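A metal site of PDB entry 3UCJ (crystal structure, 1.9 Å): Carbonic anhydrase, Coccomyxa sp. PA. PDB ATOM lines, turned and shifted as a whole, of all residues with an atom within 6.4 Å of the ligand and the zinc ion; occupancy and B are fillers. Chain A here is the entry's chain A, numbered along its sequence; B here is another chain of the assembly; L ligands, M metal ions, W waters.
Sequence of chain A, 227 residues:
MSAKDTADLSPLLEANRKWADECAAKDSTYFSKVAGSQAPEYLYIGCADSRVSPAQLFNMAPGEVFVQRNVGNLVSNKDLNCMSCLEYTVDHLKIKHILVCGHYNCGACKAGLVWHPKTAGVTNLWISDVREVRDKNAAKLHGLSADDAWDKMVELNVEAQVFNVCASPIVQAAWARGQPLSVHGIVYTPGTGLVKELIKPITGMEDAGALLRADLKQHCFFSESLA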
ATOM      1  N   CYS A  47       5.661  18.677   6.374  1.00  0.00           N
ATOM      2  CA  CYS A  47       4.230  18.871   6.700  1.00  0.00           C
ATOM      3  C   CYS A  47       3.458  19.557   5.568  1.00  0.00           C
ATOM      4  O   CYS A  47       4.056  20.425   4.883  1.00  0.00           O
ATOM      5  CB  CYS A  47       4.107  19.708   8.027  1.00  0.00           C
ATOM      6  SG  CYS A  47       2.397  19.616   8.515  1.00  0.00           S
ATOM      7  N   ALA A  48       2.159  19.256   5.390  1.00  0.00           N
ATOM      8  CA  ALA A  48       1.329  19.801   4.409  1.00  0.00           C
ATOM      9  C   ALA A  48       0.974  21.305   4.724  1.00  0.00           C
ATOM     10  O   ALA A  48       0.473  21.976   3.899  1.00  0.00           O
ATOM     11  CB  ALA A  48       0.022  18.961   4.296  1.00  0.00           C
ATOM     12  N   ASP A  49       1.303  21.756   5.929  1.00  0.00           N
ATOM     13  CA  ASP A  49       1.066  23.162   6.390  1.00  0.00           C
ATOM     14  C   ASP A  49       1.477  24.177   5.308  1.00  0.00           C
ATOM     15  O   ASP A  49       2.590  24.110   4.793  1.00  0.00           O
ATOM     16  CB  ASP A  49       1.941  23.358   7.625  1.00  0.00           C
ATOM     17  CG  ASP A  49       1.617  24.691   8.373  1.00  0.00           C
ATOM     18  OD1 ASP A  49       1.754  25.758   7.751  1.00  0.00           O
ATOM     19  OD2 ASP A  49       1.125  24.611   9.516  1.00  0.00           O
ATOM     20  N   SER A  50       0.541  25.040   4.956  1.00  0.00           N
ATOM     21  CA  SER A  50       0.671  26.062   3.913  1.00  0.00           C
ATOM     22  C   SER A  50       1.823  27.042   4.120  1.00  0.00           C
ATOM     23  O   SER A  50       2.123  27.795   3.186  1.00  0.00           O
ATOM     24  CB  SER A  50      -0.643  26.869   3.791  1.00  0.00           C
ATOM     25  OG  SER A  50      -0.870  27.643   4.971  1.00  0.00           O
ATOM     26  N   ARG A  51       2.462  27.018   5.293  1.00  0.00           N
ATOM     27  CA  ARG A  51       3.521  27.976   5.560  1.00  0.00           C
ATOM     28  C   ARG A  51       4.893  27.428   5.251  1.00  0.00           C
ATOM     29  O   ARG A  51       5.927  28.122   5.488  1.00  0.00           O
ATOM     30  CB  ARG A  51       3.432  28.434   7.002  1.00  0.00           C
ATOM     31  CG  ARG A  51       2.192  29.197   7.203  1.00  0.00           C
ATOM     32  CD  ARG A  51       1.929  29.363   8.717  1.00  0.00           C
ATOM     33  NE  ARG A  51       1.719  28.080   9.437  1.00  0.00           N
ATOM     34  CZ  ARG A  51       1.715  27.961  10.766  1.00  0.00           C
ATOM     35  NH1 ARG A  51       1.961  29.034  11.574  1.00  0.00           N
ATOM     36  NH2 ARG A  51       1.562  26.743  11.305  1.00  0.00           N
ATOM     37  N   VAL A  52       4.924  26.176   4.773  1.00  0.00           N
ATOM     38  CA  VAL A  52       6.193  25.446   4.737  1.00  0.00           C
ATOM     39  C   VAL A  52       6.460  24.829   3.337  1.00  0.00           C
ATOM     40  O   VAL A  52       6.160  23.622   3.103  1.00  0.00           O
ATOM     41  CB  VAL A  52       6.254  24.304   5.796  1.00  0.00           C
ATOM     42  CG1 VAL A  52       7.695  23.769   5.971  1.00  0.00           C
ATOM     43  CG2 VAL A  52       5.628  24.796   7.172  1.00  0.00           C
ATOM     44  N   ASN A  70       2.609  15.634   4.101  1.00  0.00           N
ATOM     45  CA  ASN A  70       1.332  15.129   4.689  1.00  0.00           C
ATOM     46  C   ASN A  70       1.133  15.805   6.041  1.00  0.00           C
ATOM     47  O   ASN A  70       2.036  16.499   6.532  1.00  0.00           O
ATOM     48  CB  ASN A  70       1.407  13.569   4.819  1.00  0.00           C
ATOM     49  CG  ASN A  70       2.490  13.108   5.818  1.00  0.00           C
ATOM     50  OD1 ASN A  70       2.492  13.437   7.020  1.00  0.00           O
ATOM     51  ND2 ASN A  70       3.405  12.260   5.332  1.00  0.00           N
ATOM     52  N   VAL A  71      -0.040  15.628   6.623  1.00  0.00           N
ATOM     53  CA  VAL A  71      -0.286  16.266   7.950  1.00  0.00           C
ATOM     54  C   VAL A  71       0.595  15.716   9.049  1.00  0.00           C
ATOM     55  O   VAL A  71       0.548  14.511   9.426  1.00  0.00           O
ATOM     56  CB  VAL A  71      -1.845  16.106   8.304  1.00  0.00           C
ATOM     57  CG1 VAL A  71      -2.039  16.362   9.834  1.00  0.00           C
ATOM     58  CG2 VAL A  71      -2.715  16.929   7.337  1.00  0.00           C
ATOM     59  N   GLY A  72       1.459  16.585   9.613  1.00  0.00           N
ATOM     60  CA  GLY A  72       2.401  16.105  10.601  1.00  0.00           C
ATOM     61  C   GLY A  72       3.703  15.456  10.118  1.00  0.00           C
ATOM     62  O   GLY A  72       4.426  14.990  10.929  1.00  0.00           O
ATOM     63  N   ASN A  73       4.007  15.400   8.800  1.00  0.00           N
ATOM     64  CA  ASN A  73       5.261  14.886   8.355  1.00  0.00           C
ATOM     65  C   ASN A  73       5.589  13.508   8.909  1.00  0.00           C
ATOM     66  O   ASN A  73       6.657  13.220   9.416  1.00  0.00           O
ATOM     67  CB  ASN A  73       6.441  15.919   8.495  1.00  0.00           C
ATOM     68  CG  ASN A  73       6.662  16.467   9.913  1.00  0.00           C
ATOM     69  OD1 ASN A  73       6.191  17.592  10.240  1.00  0.00           O
ATOM     70  ND2 ASN A  73       7.455  15.782  10.693  1.00  0.00           N
ATOM     71  N   HIS A 103       8.030  21.208  11.738  1.00  0.00           N
ATOM     72  CA  HIS A 103       8.019  22.686  11.876  1.00  0.00           C
ATOM     73  C   HIS A 103       7.347  23.120  13.204  1.00  0.00           C
ATOM     74  O   HIS A 103       6.356  22.529  13.670  1.00  0.00           O
ATOM     75  CB  HIS A 103       7.308  23.347  10.697  1.00  0.00           C
ATOM     76  CG  HIS A 103       5.831  23.102  10.674  1.00  0.00           C
ATOM     77  ND1 HIS A 103       4.885  24.007  11.117  1.00  0.00           N
ATOM     78  CD2 HIS A 103       5.132  22.015  10.249  1.00  0.00           C
ATOM     79  CE1 HIS A 103       3.665  23.501  10.926  1.00  0.00           C
ATOM     80  NE2 HIS A 103       3.796  22.298  10.401  1.00  0.00           N
ATOM     81  N   ASN A 105       4.904  25.336  15.625  1.00  0.00           N
ATOM     82  CA  ASN A 105       3.550  25.784  15.374  1.00  0.00           C
ATOM     83  C   ASN A 105       2.750  24.780  14.477  1.00  0.00           C
ATOM     84  O   ASN A 105       1.806  25.158  13.780  1.00  0.00           O
ATOM     85  CB  ASN A 105       3.452  27.270  14.833  1.00  0.00           C
ATOM     86  CG  ASN A 105       2.096  27.891  15.100  1.00  0.00           C
ATOM     87  OD1 ASN A 105       1.315  28.199  14.172  1.00  0.00           O
ATOM     88  ND2 ASN A 105       1.816  28.191  16.402  1.00  0.00           N
ATOM     89  N   CYS A 106       3.124  23.509  14.560  1.00  0.00           N
ATOM     90  CA  CYS A 106       2.504  22.433  13.756  1.00  0.00           C
ATOM     91  C   CYS A 106       1.272  21.995  14.514  1.00  0.00           C
ATOM     92  O   CYS A 106       1.400  21.362  15.550  1.00  0.00           O
ATOM     93  CB  CYS A 106       3.494  21.271  13.636  1.00  0.00           C
ATOM     94  SG  CYS A 106       2.665  19.865  12.665  1.00  0.00           S
ATOM     95  N   GLY A 107       0.139  22.384  14.005  1.00  0.00           N
ATOM     96  CA  GLY A 107      -1.120  22.003  14.544  1.00  0.00           C
ATOM     97  C   GLY A 107      -1.353  20.509  14.611  1.00  0.00           C
ATOM     98  O   GLY A 107      -2.139  20.063  15.477  1.00  0.00           O
ATOM     99  N   ALA A 108      -0.671  19.730  13.772  1.00  0.00           N
ATOM    100  CA  ALA A 108      -0.876  18.281  13.884  1.00  0.00           C
ATOM    101  C   ALA A 108      -0.236  17.808  15.148  1.00  0.00           C
ATOM    102  O   ALA A 108      -0.748  16.906  15.824  1.00  0.00           O
ATOM    103  CB  ALA A 108      -0.231  17.509  12.612  1.00  0.00           C
ATOM    104  N   CYS A 109       0.949  18.361  15.490  1.00  0.00           N
ATOM    105  CA  CYS A 109       1.613  17.976  16.707  1.00  0.00           C
ATOM    106  C   CYS A 109       0.838  18.434  17.937  1.00  0.00           C
ATOM    107  O   CYS A 109       0.821  17.733  18.947  1.00  0.00           O
ATOM    108  CB  CYS A 109       3.028  18.560  16.818  1.00  0.00           C
ATOM    109  SG  CYS A 109       4.133  17.606  15.633  1.00  0.00           S
ATOM    110  N   ALA A 111      -2.522  18.888  18.081  1.00  0.00           N
ATOM    111  CA  ALA A 111      -3.672  17.992  18.167  1.00  0.00           C
ATOM    112  C   ALA A 111      -3.243  16.623  18.743  1.00  0.00           C
ATOM    113  O   ALA A 111      -3.932  16.049  19.565  1.00  0.00           O
ATOM    114  CB  ALA A 111      -4.344  17.853  16.790  1.00  0.00           C
ATOM    115  N   TRP A 115      -5.778  16.271  21.654  1.00  0.00           N
ATOM    116  CA  TRP A 115      -7.082  15.709  21.327  1.00  0.00           C
ATOM    117  C   TRP A 115      -7.335  14.427  22.137  1.00  0.00           C
ATOM    118  O   TRP A 115      -6.393  13.584  22.359  1.00  0.00           O
ATOM    119  CB  TRP A 115      -7.215  15.350  19.839  1.00  0.00           C
ATOM    120  CG  TRP A 115      -7.501  16.522  18.929  1.00  0.00           C
ATOM    121  CD1 TRP A 115      -7.451  17.900  19.267  1.00  0.00           C
ATOM    122  CD2 TRP A 115      -7.942  16.481  17.581  1.00  0.00           C
ATOM    123  NE1 TRP A 115      -7.783  18.653  18.171  1.00  0.00           N
ATOM    124  CE2 TRP A 115      -8.104  17.825  17.132  1.00  0.00           C
ATOM    125  CE3 TRP A 115      -8.228  15.422  16.684  1.00  0.00           C
ATOM    126  CZ2 TRP A 115      -8.551  18.125  15.818  1.00  0.00           C
ATOM    127  CZ3 TRP A 115      -8.637  15.705  15.424  1.00  0.00           C
ATOM    128  CH2 TRP A 115      -8.826  17.031  14.981  1.00  0.00           C
ATOM    129  N   THR A 123      -8.633  12.767  10.211  1.00  0.00           N
ATOM    130  CA  THR A 123      -7.433  13.355  10.675  1.00  0.00           C
ATOM    131  C   THR A 123      -7.034  12.787  12.041  1.00  0.00           C
ATOM    132  O   THR A 123      -5.852  12.565  12.334  1.00  0.00           O
ATOM    133  CB  THR A 123      -7.578  14.911  10.798  1.00  0.00           C
ATOM    134  OG1 THR A 123      -7.993  15.438   9.539  1.00  0.00           O
ATOM    135  CG2 THR A 123      -6.260  15.548  11.177  1.00  0.00           C
ATOM    136  N   ASN A 124      -8.027  12.579  12.903  1.00  0.00           N
ATOM    137  CA  ASN A 124      -7.738  12.036  14.208  1.00  0.00           C
ATOM    138  C   ASN A 124      -7.101  10.561  14.049  1.00  0.00           C
ATOM    139  O   ASN A 124      -6.207  10.197  14.774  1.00  0.00           O
ATOM    140  CB  ASN A 124      -9.026  11.909  15.083  1.00  0.00           C
ATOM    141  CG  ASN A 124      -8.672  11.303  16.447  1.00  0.00           C
ATOM    142  OD1 ASN A 124      -7.855  11.843  17.226  1.00  0.00           O
ATOM    143  ND2 ASN A 124      -9.212  10.141  16.710  1.00  0.00           N
ATOM    144  N   ILE A 127      -3.302  11.148  12.844  1.00  0.00           N
ATOM    145  CA  ILE A 127      -2.295  11.523  13.776  1.00  0.00           C
ATOM    146  C   ILE A 127      -2.100  10.561  14.928  1.00  0.00           C
ATOM    147  O   ILE A 127      -1.349  10.877  15.858  1.00  0.00           O
ATOM    148  CB  ILE A 127      -2.651  13.032  14.339  1.00  0.00           C
ATOM    149  CG1 ILE A 127      -3.942  12.907  15.170  1.00  0.00           C
ATOM    150  CG2 ILE A 127      -2.706  13.981  13.134  1.00  0.00           C
ATOM    151  CD1 ILE A 127      -4.221  14.306  15.972  1.00  0.00           C
ATOM    152  N   GLN B  38      -2.490  30.000  10.096  1.00  0.00           N
ATOM    153  CA  GLN B  38      -2.511  29.995   8.618  1.00  0.00           C
ATOM    154  C   GLN B  38      -3.930  30.114   8.224  1.00  0.00           C
ATOM    155  O   GLN B  38      -4.833  29.597   8.893  1.00  0.00           O
ATOM    156  CB  GLN B  38      -1.914  28.685   8.013  1.00  0.00           C
ATOM    157  CG  GLN B  38      -2.754  27.396   8.462  1.00  0.00           C
ATOM    158  CD  GLN B  38      -2.070  26.061   8.014  1.00  0.00           C
ATOM    159  OE1 GLN B  38      -1.589  25.928   6.856  1.00  0.00           O
ATOM    160  NE2 GLN B  38      -2.077  25.076   8.895  1.00  0.00           N
ATOM    161  N   PHE B  66      -1.991  25.079   1.034  1.00  0.00           N
ATOM    162  CA  PHE B  66      -1.751  23.869   1.803  1.00  0.00           C
ATOM    163  C   PHE B  66      -1.534  22.747   0.739  1.00  0.00           C
ATOM    164  O   PHE B  66      -2.242  22.725  -0.250  1.00  0.00           O
ATOM    165  CB  PHE B  66      -3.058  23.594   2.550  1.00  0.00           C
ATOM    166  CG  PHE B  66      -2.914  22.630   3.696  1.00  0.00           C
ATOM    167  CD1 PHE B  66      -2.752  23.105   5.013  1.00  0.00           C
ATOM    168  CD2 PHE B  66      -3.072  21.236   3.506  1.00  0.00           C
ATOM    169  CE1 PHE B  66      -2.690  22.247   6.083  1.00  0.00           C
ATOM    170  CE2 PHE B  66      -2.979  20.330   4.625  1.00  0.00           C
ATOM    171  CZ  PHE B  66      -2.771  20.814   5.893  1.00  0.00           C
ATOM    172  N   TYR B  88      -8.743  18.253   6.910  1.00  0.00           N
ATOM    173  CA  TYR B  88      -8.302  19.417   7.655  1.00  0.00           C
ATOM    174  C   TYR B  88      -8.515  20.750   6.940  1.00  0.00           C
ATOM    175  O   TYR B  88      -8.886  21.701   7.559  1.00  0.00           O
ATOM    176  CB  TYR B  88      -6.866  19.303   8.143  1.00  0.00           C
ATOM    177  CG  TYR B  88      -6.474  20.456   9.018  1.00  0.00           C
ATOM    178  CD1 TYR B  88      -7.085  20.680  10.238  1.00  0.00           C
ATOM    179  CD2 TYR B  88      -5.523  21.355   8.617  1.00  0.00           C
ATOM    180  CE1 TYR B  88      -6.748  21.729  11.004  1.00  0.00           C
ATOM    181  CE2 TYR B  88      -5.186  22.403   9.383  1.00  0.00           C
ATOM    182  CZ  TYR B  88      -5.797  22.612  10.571  1.00  0.00           C
ATOM    183  OH  TYR B  88      -5.463  23.682  11.338  1.00  0.00           O
ATOM    184  N   HIS B  92     -11.678  22.437   8.678  1.00  0.00           N
ATOM    185  CA  HIS B  92     -11.177  23.278   9.706  1.00  0.00           C
ATOM    186  C   HIS B  92     -10.659  24.600   9.108  1.00  0.00           C
ATOM    187  O   HIS B  92     -11.067  25.631   9.545  1.00  0.00           O
ATOM    188  CB  HIS B  92     -10.068  22.562  10.450  1.00  0.00           C
ATOM    189  CG  HIS B  92     -10.509  21.421  11.325  1.00  0.00           C
ATOM    190  ND1 HIS B  92     -10.423  21.478  12.706  1.00  0.00           N
ATOM    191  CD2 HIS B  92     -10.930  20.170  11.028  1.00  0.00           C
ATOM    192  CE1 HIS B  92     -10.789  20.314  13.218  1.00  0.00           C
ATOM    193  NE2 HIS B  92     -11.109  19.506  12.226  1.00  0.00           N
ATOM    194  N   LEU B  93      -9.792  24.550   8.108  1.00  0.00           N
ATOM    195  CA  LEU B  93      -9.345  25.812   7.522  1.00  0.00           C
ATOM    196  C   LEU B  93     -10.340  26.491   6.621  1.00  0.00           C
ATOM    197  O   LEU B  93     -10.158  27.663   6.343  1.00  0.00           O
ATOM    198  CB  LEU B  93      -8.006  25.665   6.784  1.00  0.00           C
ATOM    199  CG  LEU B  93      -6.839  25.132   7.565  1.00  0.00           C
ATOM    200  CD1 LEU B  93      -5.600  24.931   6.627  1.00  0.00           C
ATOM    201  CD2 LEU B  93      -6.437  25.978   8.764  1.00  0.00           C
HETATM  202  C1  LIG L   1      -2.139  21.258  11.096  1.00  0.00           C
HETATM  203  C2  LIG L   1      -3.974  20.512  12.476  1.00  0.00           C
HETATM  204  C3  LIG L   1      -5.276  18.646  13.196  1.00  0.00           C
HETATM  205  C4  LIG L   1      -6.588  18.170  13.770  1.00  0.00           C
HETATM  206  N1  LIG L   1       0.544  21.774  10.619  1.00  0.00           N
HETATM  207  N2  LIG L   1      -3.608  21.819  12.710  1.00  0.00           N
HETATM  208  N3  LIG L   1      -2.482  22.302  11.856  1.00  0.00           N
HETATM  209  N4  LIG L   1      -4.944  19.932  13.342  1.00  0.00           N
HETATM  210  O1  LIG L   1      -1.172  22.181   8.855  1.00  0.00           O
HETATM  211  O2  LIG L   1      -0.634  19.975   9.644  1.00  0.00           O
HETATM  212  O3  LIG L   1      -4.485  17.876  12.576  1.00  0.00           O
HETATM  213  S1  LIG L   1      -0.841  21.433   9.943  1.00  0.00           S
HETATM  214  S2  LIG L   1      -3.085  19.762  11.246  1.00  0.00           S
HETATM  215 ZN    ZN M   1       2.266  20.886  10.510  1.00  0.00          ZN
HETATM  216  O   HOH W   1      -6.296  21.590  14.971  1.00  0.00           O
HETATM  217  O   HOH W   2      -4.469  23.483  14.529  1.00  0.00           O
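Merely in contact with the zinc ion: Asp 49. Of the 26 residues printed, 4 come within 4 Å of the zinc ion. Along chain A the residues within 4 Å of the zinc ion span positions 47 to 106. The nearest printed residue that does not touch the zinc ion is Gly 107 (4.4 Å).
The backbone NH of Ala 108 lies close to the side-chain sulfur of Cys 106, at 3.5 Å. O of Tyr 88 of chain B is in hydrogen-bond range of N of Leu 93 of chain B, 3.0 Å away. The backbone NH (N) of Gly 72 lies close to the side-chain sulfur (SG) of Cys 47, 3.4 Å away. The side-chain amide oxygen (OE1) of Gln 38 of chain B is in hydrogen-bond range of the side-chain hydroxyl (OG) of Ser 50, 2.6 Å away. N of Asp 49 sits close to SG of Cys 47 (3.5 Å). The side-chain sulfur (SG) of Cys 47 lies close to the backbone carbonyl oxygen (O) of Asn 70 (3.7 Å). The guanidinium group (NH2) of Arg 51 is in salt-bridge range of the side-chain carboxylate (OD2) of Asp 49. N of Cys 109 lies close to SG of Cys 106, at 3.6 Å.
The zinc ion is bound by a nitrogen (N1) of the ligand, a ring nitrogen (NE2) of His 103, the side-chain sulfur of Cys 47 and the side-chain sulfur of Cys 106. The zinc ion has four donor atoms within binding distance.
Water W2 lies within hydrogen-bond range of a nitrogen (N2) of the ligand (2.6 Å) and the side-chain hydroxyl (OH) of Tyr 88 of chain B (3.3 Å).
An oxygen (O1) of the ligand lies within hydrogen-bond range of the side-chain amide nitrogen (NE2) of Gln 38 of chain B (3.0 Å). The side-chain hydroxyl of Tyr 88 of chain B is in hydrogen-bond range of a nitrogen (N2) of the ligand (3.0 Å). N3 of the ligand sits close to N of Gly 107. The backbone NH (N) of Ala 108 sits close to a sulfur (S2) of the ligand. OD2 of Asp 49 lies close to N1 of the ligand.
Val 71 touches the ligand. Gly 72 touches the ligand (N to O2, 3.98 Å). CB of Ala 111 touches C4 of the ligand (3.8 Å). CH2 of Trp 115 touches C4 of the ligand (2.8 Å). Thr 123 touches the ligand. CE1 of Phe 66 of chain B touches O1 of the ligand, at 3.2 Å. Hydrophobic or aromatic side chains within 4 Å of the ligand: Val 71, His 103, Ala 108, Ala 111, Trp 115, Phe 66 of chain B and Tyr 88 of chain B. 14 residues have an atom within 4 Å of the ligand: Cys 47, Asp 49, Val 71, Gly 72, His 103, Cys 106, Gly 107, Ala 108, Ala 111, Trp 115, Thr 123, Gln 38 of chain B, Phe 66 of chain B and Tyr 88 of chain B.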
